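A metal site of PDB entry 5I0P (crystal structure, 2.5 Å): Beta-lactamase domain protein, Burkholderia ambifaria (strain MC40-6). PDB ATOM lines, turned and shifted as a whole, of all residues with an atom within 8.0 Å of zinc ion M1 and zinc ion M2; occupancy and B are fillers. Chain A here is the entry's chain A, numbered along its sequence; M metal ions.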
ATOM      1  N   LEU A  44      14.860 -15.907 -13.869  1.00  0.00           N
ATOM      2  CA  LEU A  44      13.789 -15.330 -13.080  1.00  0.00           C
ATOM      3  C   LEU A  44      13.933 -15.846 -11.657  1.00  0.00           C
ATOM      4  O   LEU A  44      14.426 -16.942 -11.461  1.00  0.00           O
ATOM      5  CB  LEU A  44      12.403 -15.681 -13.650  1.00  0.00           C
ATOM      6  CG  LEU A  44      12.117 -15.017 -15.001  1.00  0.00           C
ATOM      7  CD1 LEU A  44      10.858 -15.538 -15.581  1.00  0.00           C
ATOM      8  CD2 LEU A  44      12.049 -13.470 -14.919  1.00  0.00           C
ATOM      9  N   LEU A  48       9.214 -20.583 -11.484  1.00  0.00           N
ATOM     10  CA  LEU A  48       9.497 -20.460 -12.901  1.00  0.00           C
ATOM     11  C   LEU A  48      10.811 -19.679 -13.006  1.00  0.00           C
ATOM     12  O   LEU A  48      10.830 -18.479 -12.729  1.00  0.00           O
ATOM     13  CB  LEU A  48       8.334 -19.733 -13.564  1.00  0.00           C
ATOM     14  CG  LEU A  48       8.308 -19.590 -15.067  1.00  0.00           C
ATOM     15  CD1 LEU A  48       7.876 -20.867 -15.680  1.00  0.00           C
ATOM     16  CD2 LEU A  48       7.386 -18.417 -15.456  1.00  0.00           C
ATOM     17  N   HIS A  50      13.066 -19.006 -15.460  1.00  0.00           N
ATOM     18  CA  HIS A  50      13.644 -18.445 -16.663  1.00  0.00           C
ATOM     19  C   HIS A  50      12.535 -17.960 -17.575  1.00  0.00           C
ATOM     20  O   HIS A  50      11.410 -18.430 -17.522  1.00  0.00           O
ATOM     21  CB  HIS A  50      14.494 -19.492 -17.384  1.00  0.00           C
ATOM     22  CG  HIS A  50      13.683 -20.515 -18.097  1.00  0.00           C
ATOM     23  ND1 HIS A  50      13.210 -21.659 -17.469  1.00  0.00           N
ATOM     24  CD2 HIS A  50      13.204 -20.553 -19.368  1.00  0.00           C
ATOM     25  CE1 HIS A  50      12.510 -22.376 -18.341  1.00  0.00           C
ATOM     26  NE2 HIS A  50      12.478 -21.715 -19.491  1.00  0.00           N
ATOM     27  N   ILE A  51      12.888 -17.066 -18.484  1.00  0.00           N
ATOM     28  CA  ILE A  51      12.037 -16.765 -19.637  1.00  0.00           C
ATOM     29  C   ILE A  51      12.924 -16.715 -20.880  1.00  0.00           C
ATOM     30  O   ILE A  51      14.045 -16.208 -20.833  1.00  0.00           O
ATOM     31  CB  ILE A  51      11.246 -15.451 -19.451  1.00  0.00           C
ATOM     32  CG1 ILE A  51      10.370 -15.171 -20.686  1.00  0.00           C
ATOM     33  CG2 ILE A  51      12.146 -14.263 -19.091  1.00  0.00           C
ATOM     34  CD1 ILE A  51       9.377 -14.045 -20.509  1.00  0.00           C
ATOM     35  N   ASN A  52      12.413 -17.265 -21.974  1.00  0.00           N
ATOM     36  CA  ASN A  52      13.096 -17.223 -23.266  1.00  0.00           C
ATOM     37  C   ASN A  52      12.660 -15.978 -24.018  1.00  0.00           C
ATOM     38  O   ASN A  52      11.465 -15.727 -24.139  1.00  0.00           O
ATOM     39  CB  ASN A  52      12.808 -18.451 -24.111  1.00  0.00           C
ATOM     40  CG  ASN A  52      13.150 -19.725 -23.406  1.00  0.00           C
ATOM     41  OD1 ASN A  52      14.222 -19.817 -22.818  1.00  0.00           O
ATOM     42  ND2 ASN A  52      12.276 -20.735 -23.484  1.00  0.00           N
ATOM     43  N   ASP A  70       9.648  -9.786 -26.335  1.00  0.00           N
ATOM     44  CA  ASP A  70       9.547  -9.959 -24.881  1.00  0.00           C
ATOM     45  C   ASP A  70      10.830  -9.519 -24.174  1.00  0.00           C
ATOM     46  O   ASP A  70      11.907  -9.518 -24.755  1.00  0.00           O
ATOM     47  CB  ASP A  70       9.160 -11.407 -24.538  1.00  0.00           C
ATOM     48  CG  ASP A  70       7.683 -11.722 -24.865  1.00  0.00           C
ATOM     49  OD1 ASP A  70       6.949 -10.766 -25.163  1.00  0.00           O
ATOM     50  OD2 ASP A  70       7.263 -12.895 -24.817  1.00  0.00           O
ATOM     51  N   THR A 101       4.436 -10.331 -26.282  1.00  0.00           N
ATOM     52  CA  THR A 101       3.370 -11.303 -26.476  1.00  0.00           C
ATOM     53  C   THR A 101       2.148 -11.016 -25.610  1.00  0.00           C
ATOM     54  O   THR A 101       0.999 -11.227 -26.036  1.00  0.00           O
ATOM     55  CB  THR A 101       3.904 -12.724 -26.222  1.00  0.00           C
ATOM     56  OG1 THR A 101       4.462 -12.835 -24.902  1.00  0.00           O
ATOM     57  CG2 THR A 101       4.944 -13.119 -27.232  1.00  0.00           C
ATOM     58  N   HIS A 102       2.364 -10.585 -24.372  1.00  0.00           N
ATOM     59  CA  HIS A 102       1.265 -10.412 -23.443  1.00  0.00           C
ATOM     60  C   HIS A 102       1.847  -9.734 -22.207  1.00  0.00           C
ATOM     61  O   HIS A 102       3.066  -9.592 -22.070  1.00  0.00           O
ATOM     62  CB  HIS A 102       0.562 -11.735 -23.124  1.00  0.00           C
ATOM     63  CG  HIS A 102       1.360 -12.736 -22.332  1.00  0.00           C
ATOM     64  ND1 HIS A 102       2.479 -13.381 -22.828  1.00  0.00           N
ATOM     65  CD2 HIS A 102       1.159 -13.233 -21.090  1.00  0.00           C
ATOM     66  CE1 HIS A 102       2.933 -14.222 -21.926  1.00  0.00           C
ATOM     67  NE2 HIS A 102       2.158 -14.155 -20.858  1.00  0.00           N
ATOM     68  N   CYS A 103       0.951  -9.294 -21.309  1.00  0.00           N
ATOM     69  CA  CYS A 103       1.332  -8.298 -20.311  1.00  0.00           C
ATOM     70  C   CYS A 103       1.903  -8.875 -19.021  1.00  0.00           C
ATOM     71  O   CYS A 103       2.178  -8.106 -18.087  1.00  0.00           O
ATOM     72  CB  CYS A 103       0.143  -7.391 -19.971  1.00  0.00           C
ATOM     73  SG  CYS A 103      -1.184  -8.216 -19.052  1.00  0.00           S
ATOM     74  N   HIS A 104       2.055 -10.198 -18.912  1.00  0.00           N
ATOM     75  CA  HIS A 104       2.626 -10.733 -17.669  1.00  0.00           C
ATOM     76  C   HIS A 104       4.038 -10.193 -17.457  1.00  0.00           C
ATOM     77  O   HIS A 104       4.794  -9.957 -18.426  1.00  0.00           O
ATOM     78  CB  HIS A 104       2.608 -12.262 -17.665  1.00  0.00           C
ATOM     79  CG  HIS A 104       1.222 -12.811 -17.548  1.00  0.00           C
ATOM     80  ND1 HIS A 104       0.877 -14.077 -17.981  1.00  0.00           N
ATOM     81  CD2 HIS A 104       0.082 -12.253 -17.094  1.00  0.00           C
ATOM     82  CE1 HIS A 104      -0.417 -14.265 -17.786  1.00  0.00           C
ATOM     83  NE2 HIS A 104      -0.924 -13.175 -17.251  1.00  0.00           N
ATOM     84  N   PRO A 105       4.399  -9.965 -16.195  1.00  0.00           N
ATOM     85  CA  PRO A 105       5.598  -9.153 -15.889  1.00  0.00           C
ATOM     86  C   PRO A 105       6.904  -9.701 -16.498  1.00  0.00           C
ATOM     87  O   PRO A 105       7.799  -8.911 -16.849  1.00  0.00           O
ATOM     88  CB  PRO A 105       5.644  -9.185 -14.365  1.00  0.00           C
ATOM     89  CG  PRO A 105       4.320  -9.601 -13.950  1.00  0.00           C
ATOM     90  CD  PRO A 105       3.762 -10.481 -14.988  1.00  0.00           C
ATOM     91  N   ASP A 106       7.046 -11.032 -16.590  1.00  0.00           N
ATOM     92  CA  ASP A 106       8.278 -11.564 -17.141  1.00  0.00           C
ATOM     93  C   ASP A 106       8.392 -11.284 -18.644  1.00  0.00           C
ATOM     94  O   ASP A 106       9.509 -11.280 -19.171  1.00  0.00           O
ATOM     95  CB  ASP A 106       8.427 -13.073 -16.800  1.00  0.00           C
ATOM     96  CG  ASP A 106       7.150 -13.905 -17.043  1.00  0.00           C
ATOM     97  OD1 ASP A 106       7.271 -15.064 -17.533  1.00  0.00           O
ATOM     98  OD2 ASP A 106       6.029 -13.440 -16.741  1.00  0.00           O
ATOM     99  N   HIS A 107       7.273 -10.975 -19.332  1.00  0.00           N
ATOM    100  CA  HIS A 107       7.352 -10.629 -20.750  1.00  0.00           C
ATOM    101  C   HIS A 107       7.439  -9.134 -21.005  1.00  0.00           C
ATOM    102  O   HIS A 107       8.110  -8.730 -21.959  1.00  0.00           O
ATOM    103  CB  HIS A 107       6.147 -11.209 -21.492  1.00  0.00           C
ATOM    104  CG  HIS A 107       6.053 -12.690 -21.365  1.00  0.00           C
ATOM    105  ND1 HIS A 107       6.360 -13.560 -22.398  1.00  0.00           N
ATOM    106  CD2 HIS A 107       5.741 -13.477 -20.305  1.00  0.00           C
ATOM    107  CE1 HIS A 107       6.201 -14.797 -21.994  1.00  0.00           C
ATOM    108  NE2 HIS A 107       5.824 -14.778 -20.735  1.00  0.00           N
ATOM    109  N   GLU A 133      -3.725  -6.612 -24.060  1.00  0.00           N
ATOM    110  CA  GLU A 133      -2.577  -6.783 -23.177  1.00  0.00           C
ATOM    111  C   GLU A 133      -2.008  -5.442 -22.755  1.00  0.00           C
ATOM    112  O   GLU A 133      -1.751  -5.221 -21.567  1.00  0.00           O
ATOM    113  CB  GLU A 133      -1.497  -7.623 -23.873  1.00  0.00           C
ATOM    114  CG  GLU A 133      -1.975  -9.006 -24.296  1.00  0.00           C
ATOM    115  CD  GLU A 133      -2.188  -9.927 -23.098  1.00  0.00           C
ATOM    116  OE1 GLU A 133      -1.632  -9.621 -22.012  1.00  0.00           O
ATOM    117  OE2 GLU A 133      -2.886 -10.968 -23.247  1.00  0.00           O
ATOM    118  N   HIS A 213      -5.367 -17.373 -20.844  1.00  0.00           N
ATOM    119  CA  HIS A 213      -4.172 -17.082 -20.047  1.00  0.00           C
ATOM    120  C   HIS A 213      -4.042 -15.593 -19.743  1.00  0.00           C
ATOM    121  O   HIS A 213      -3.651 -15.210 -18.641  1.00  0.00           O
ATOM    122  CB  HIS A 213      -2.945 -17.634 -20.777  1.00  0.00           C
ATOM    123  CG  HIS A 213      -1.648 -17.327 -20.097  1.00  0.00           C
ATOM    124  ND1 HIS A 213      -1.287 -17.878 -18.883  1.00  0.00           N
ATOM    125  CD2 HIS A 213      -0.593 -16.579 -20.506  1.00  0.00           C
ATOM    126  CE1 HIS A 213      -0.090 -17.425 -18.546  1.00  0.00           C
ATOM    127  NE2 HIS A 213       0.359 -16.654 -19.509  1.00  0.00           N
ATOM    128  N   SER A 214      -4.428 -14.752 -20.689  1.00  0.00           N
ATOM    129  CA  SER A 214      -4.274 -13.298 -20.613  1.00  0.00           C
ATOM    130  C   SER A 214      -5.285 -12.680 -21.565  1.00  0.00           C
ATOM    131  O   SER A 214      -5.917 -13.400 -22.360  1.00  0.00           O
ATOM    132  CB  SER A 214      -2.844 -12.874 -20.967  1.00  0.00           C
ATOM    133  OG  SER A 214      -2.505 -13.252 -22.292  1.00  0.00           O
ATOM    134  N   HIS A 217      -3.537 -12.716 -25.996  1.00  0.00           N
ATOM    135  CA  HIS A 217      -2.150 -13.145 -26.065  1.00  0.00           C
ATOM    136  C   HIS A 217      -1.673 -13.217 -27.503  1.00  0.00           C
ATOM    137  O   HIS A 217      -2.338 -13.788 -28.371  1.00  0.00           O
ATOM    138  CB  HIS A 217      -2.003 -14.509 -25.382  1.00  0.00           C
ATOM    139  CG  HIS A 217      -0.610 -15.057 -25.421  1.00  0.00           C
ATOM    140  ND1 HIS A 217      -0.068 -15.620 -26.565  1.00  0.00           N
ATOM    141  CD2 HIS A 217       0.334 -15.156 -24.455  1.00  0.00           C
ATOM    142  CE1 HIS A 217       1.169 -16.013 -26.298  1.00  0.00           C
ATOM    143  NE2 HIS A 217       1.431 -15.763 -25.029  1.00  0.00           N
ATOM    144  N   GLY A 231       4.774 -17.890 -27.042  1.00  0.00           N
ATOM    145  CA  GLY A 231       4.476 -17.178 -25.803  1.00  0.00           C
ATOM    146  C   GLY A 231       4.272 -18.172 -24.679  1.00  0.00           C
ATOM    147  O   GLY A 231       5.020 -19.149 -24.538  1.00  0.00           O
ATOM    148  N   ASP A 232       3.238 -17.967 -23.885  1.00  0.00           N
ATOM    149  CA  ASP A 232       2.899 -18.910 -22.835  1.00  0.00           C
ATOM    150  C   ASP A 232       1.757 -19.841 -23.241  1.00  0.00           C
ATOM    151  O   ASP A 232       1.306 -20.615 -22.407  1.00  0.00           O
ATOM    152  CB  ASP A 232       2.490 -18.197 -21.556  1.00  0.00           C
ATOM    153  CG  ASP A 232       3.643 -17.559 -20.809  1.00  0.00           C
ATOM    154  OD1 ASP A 232       4.834 -17.685 -21.130  1.00  0.00           O
ATOM    155  OD2 ASP A 232       3.321 -16.875 -19.830  1.00  0.00           O
ATOM    156  N   MET A 233       1.279 -19.789 -24.493  1.00  0.00           N
ATOM    157  CA  MET A 233       0.100 -20.583 -24.831  1.00  0.00           C
ATOM    158  C   MET A 233       0.445 -22.064 -24.968  1.00  0.00           C
ATOM    159  O   MET A 233      -0.364 -22.928 -24.578  1.00  0.00           O
ATOM    160  CB  MET A 233      -0.566 -20.053 -26.111  1.00  0.00           C
ATOM    161  CG  MET A 233      -1.172 -18.704 -25.920  1.00  0.00           C
ATOM    162  SD  MET A 233      -2.590 -18.730 -24.790  1.00  0.00           S
ATOM    163  CE  MET A 233      -3.792 -19.716 -25.688  1.00  0.00           C
ATOM    164  N   LEU A 235       3.533 -24.459 -23.797  1.00  0.00           N
ATOM    165  CA  LEU A 235       4.807 -24.656 -23.160  1.00  0.00           C
ATOM    166  C   LEU A 235       5.129 -26.161 -23.101  1.00  0.00           C
ATOM    167  O   LEU A 235       4.243 -26.975 -22.851  1.00  0.00           O
ATOM    168  CB  LEU A 235       4.817 -24.062 -21.755  1.00  0.00           C
ATOM    169  CG  LEU A 235       4.397 -22.596 -21.719  1.00  0.00           C
ATOM    170  CD1 LEU A 235       4.179 -22.133 -20.257  1.00  0.00           C
ATOM    171  CD2 LEU A 235       5.388 -21.738 -22.412  1.00  0.00           C
ATOM    172  N   ILE A 238       5.541 -27.326 -18.863  1.00  0.00           N
ATOM    173  CA  ILE A 238       4.643 -26.916 -17.796  1.00  0.00           C
ATOM    174  C   ILE A 238       3.308 -26.508 -18.406  1.00  0.00           C
ATOM    175  O   ILE A 238       3.223 -26.121 -19.567  1.00  0.00           O
ATOM    176  CB  ILE A 238       5.233 -25.772 -16.969  1.00  0.00           C
ATOM    177  CG1 ILE A 238       5.294 -24.507 -17.779  1.00  0.00           C
ATOM    178  CG2 ILE A 238       6.682 -26.092 -16.563  1.00  0.00           C
ATOM    179  CD1 ILE A 238       5.926 -23.380 -17.027  1.00  0.00           C
ATOM    180  N   THR A 240      -0.045 -24.086 -18.904  1.00  0.00           N
ATOM    181  CA  THR A 240      -0.265 -22.651 -18.956  1.00  0.00           C
ATOM    182  C   THR A 240      -1.217 -22.231 -17.844  1.00  0.00           C
ATOM    183  O   THR A 240      -2.259 -22.875 -17.642  1.00  0.00           O
ATOM    184  CB  THR A 240      -0.859 -22.256 -20.315  1.00  0.00           C
ATOM    185  OG1 THR A 240       0.070 -22.582 -21.353  1.00  0.00           O
ATOM    186  CG2 THR A 240      -1.210 -20.795 -20.357  1.00  0.00           C
ATOM    187  N   ASN A 241      -0.863 -21.186 -17.102  1.00  0.00           N
ATOM    188  CA  ASN A 241      -1.754 -20.732 -16.046  1.00  0.00           C
ATOM    189  C   ASN A 241      -3.072 -20.220 -16.614  1.00  0.00           C
ATOM    190  O   ASN A 241      -3.095 -19.442 -17.571  1.00  0.00           O
ATOM    191  CB  ASN A 241      -1.132 -19.640 -15.197  1.00  0.00           C
ATOM    192  CG  ASN A 241      -2.127 -19.152 -14.157  1.00  0.00           C
ATOM    193  OD1 ASN A 241      -2.376 -19.850 -13.171  1.00  0.00           O
ATOM    194  ND2 ASN A 241      -2.744 -17.996 -14.397  1.00  0.00           N
ATOM    195  N   PRO A 275       8.937 -21.570 -27.266  1.00  0.00           N
ATOM    196  CA  PRO A 275       8.116 -21.220 -26.116  1.00  0.00           C
ATOM    197  C   PRO A 275       8.898 -20.335 -25.164  1.00  0.00           C
ATOM    198  O   PRO A 275      10.130 -20.342 -25.118  1.00  0.00           O
ATOM    199  CB  PRO A 275       7.849 -22.574 -25.458  1.00  0.00           C
ATOM    200  CG  PRO A 275       9.236 -23.279 -25.669  1.00  0.00           C
ATOM    201  CD  PRO A 275       9.746 -22.785 -27.025  1.00  0.00           C
ATOM    202  N   SER A 276       8.148 -19.570 -24.370  1.00  0.00           N
ATOM    203  CA  SER A 276       8.801 -18.638 -23.477  1.00  0.00           C
ATOM    204  C   SER A 276       9.394 -19.310 -22.247  1.00  0.00           C
ATOM    205  O   SER A 276      10.158 -18.679 -21.530  1.00  0.00           O
ATOM    206  CB  SER A 276       7.842 -17.526 -23.112  1.00  0.00           C
ATOM    207  OG  SER A 276       7.666 -16.745 -24.297  1.00  0.00           O
ATOM    208  N   HIS A 277       9.054 -20.570 -21.989  1.00  0.00           N
ATOM    209  CA  HIS A 277       9.620 -21.335 -20.887  1.00  0.00           C
ATOM    210  C   HIS A 277       9.790 -22.774 -21.344  1.00  0.00           C
ATOM    211  O   HIS A 277       8.855 -23.344 -21.911  1.00  0.00           O
ATOM    212  CB  HIS A 277       8.750 -21.226 -19.620  1.00  0.00           C
ATOM    213  CG  HIS A 277       8.297 -19.824 -19.326  1.00  0.00           C
ATOM    214  ND1 HIS A 277       9.045 -18.929 -18.597  1.00  0.00           N
ATOM    215  CD2 HIS A 277       7.159 -19.166 -19.663  1.00  0.00           C
ATOM    216  CE1 HIS A 277       8.389 -17.781 -18.493  1.00  0.00           C
ATOM    217  NE2 HIS A 277       7.249 -17.901 -19.141  1.00  0.00           N
HETATM  218 ZN    ZN M   1       5.563 -16.373 -19.107  1.00  0.00          ZN
HETATM  219 ZN    ZN M   2       2.166 -15.455 -18.827  1.00  0.00          ZN
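Of the 27 residues printed, 4 come within 4 Å of zinc ion M2.
A ring nitrogen (NE2) of His 217 sits at hydrogen-bond distance from the backbone NH (N) of Asp 232 (3.1 Å).
The backbone carbonyl oxygen of Asp 232 sits at hydrogen-bond distance from the side-chain hydroxyl of Thr 240, 2.6 Å away.
ND1 of His 213 sits at hydrogen-bond distance from O of Asn 241 (2.7 Å).
The side-chain carboxylate of Asp 106 sits close to a ring nitrogen (NE2) of His 277, 3.3 Å away.
A ring nitrogen (ND1) of His 107 is in hydrogen-bond range of the side-chain hydroxyl of Thr 101 (3.2 Å).
A ring nitrogen (ND1) of His 107 sits at hydrogen-bond distance from the side-chain carboxylate of Asp 70.
NE2 of His 217 sits close to ND1 of His 102, 3.4 Å away.
A ring nitrogen (ND1) of His 102 lies within hydrogen-bond range of the side-chain hydroxyl of Thr 101, at 2.9 Å.
Zinc ion M1 is bound by NE2 of His 277 (2.3 Å), NE2 of His 107 (2.3 Å), OD2 of Asp 232 (2.4 Å) and OD1 of Asp 232 (2.5 Å).
Slightly farther from zinc ion M1 lies OD1 of Asp 106 (2.7 Å).
Zinc ion M2 is bound by ND1 of His 104, OD2 of Asp 232, NE2 of His 213 and NE2 of His 102.
Zinc ion M2 has four donor atoms within binding distance.
Four residues have an atom within 4 Å of zinc ion M1: Asp 106, His 107, Asp 232 and His 277.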
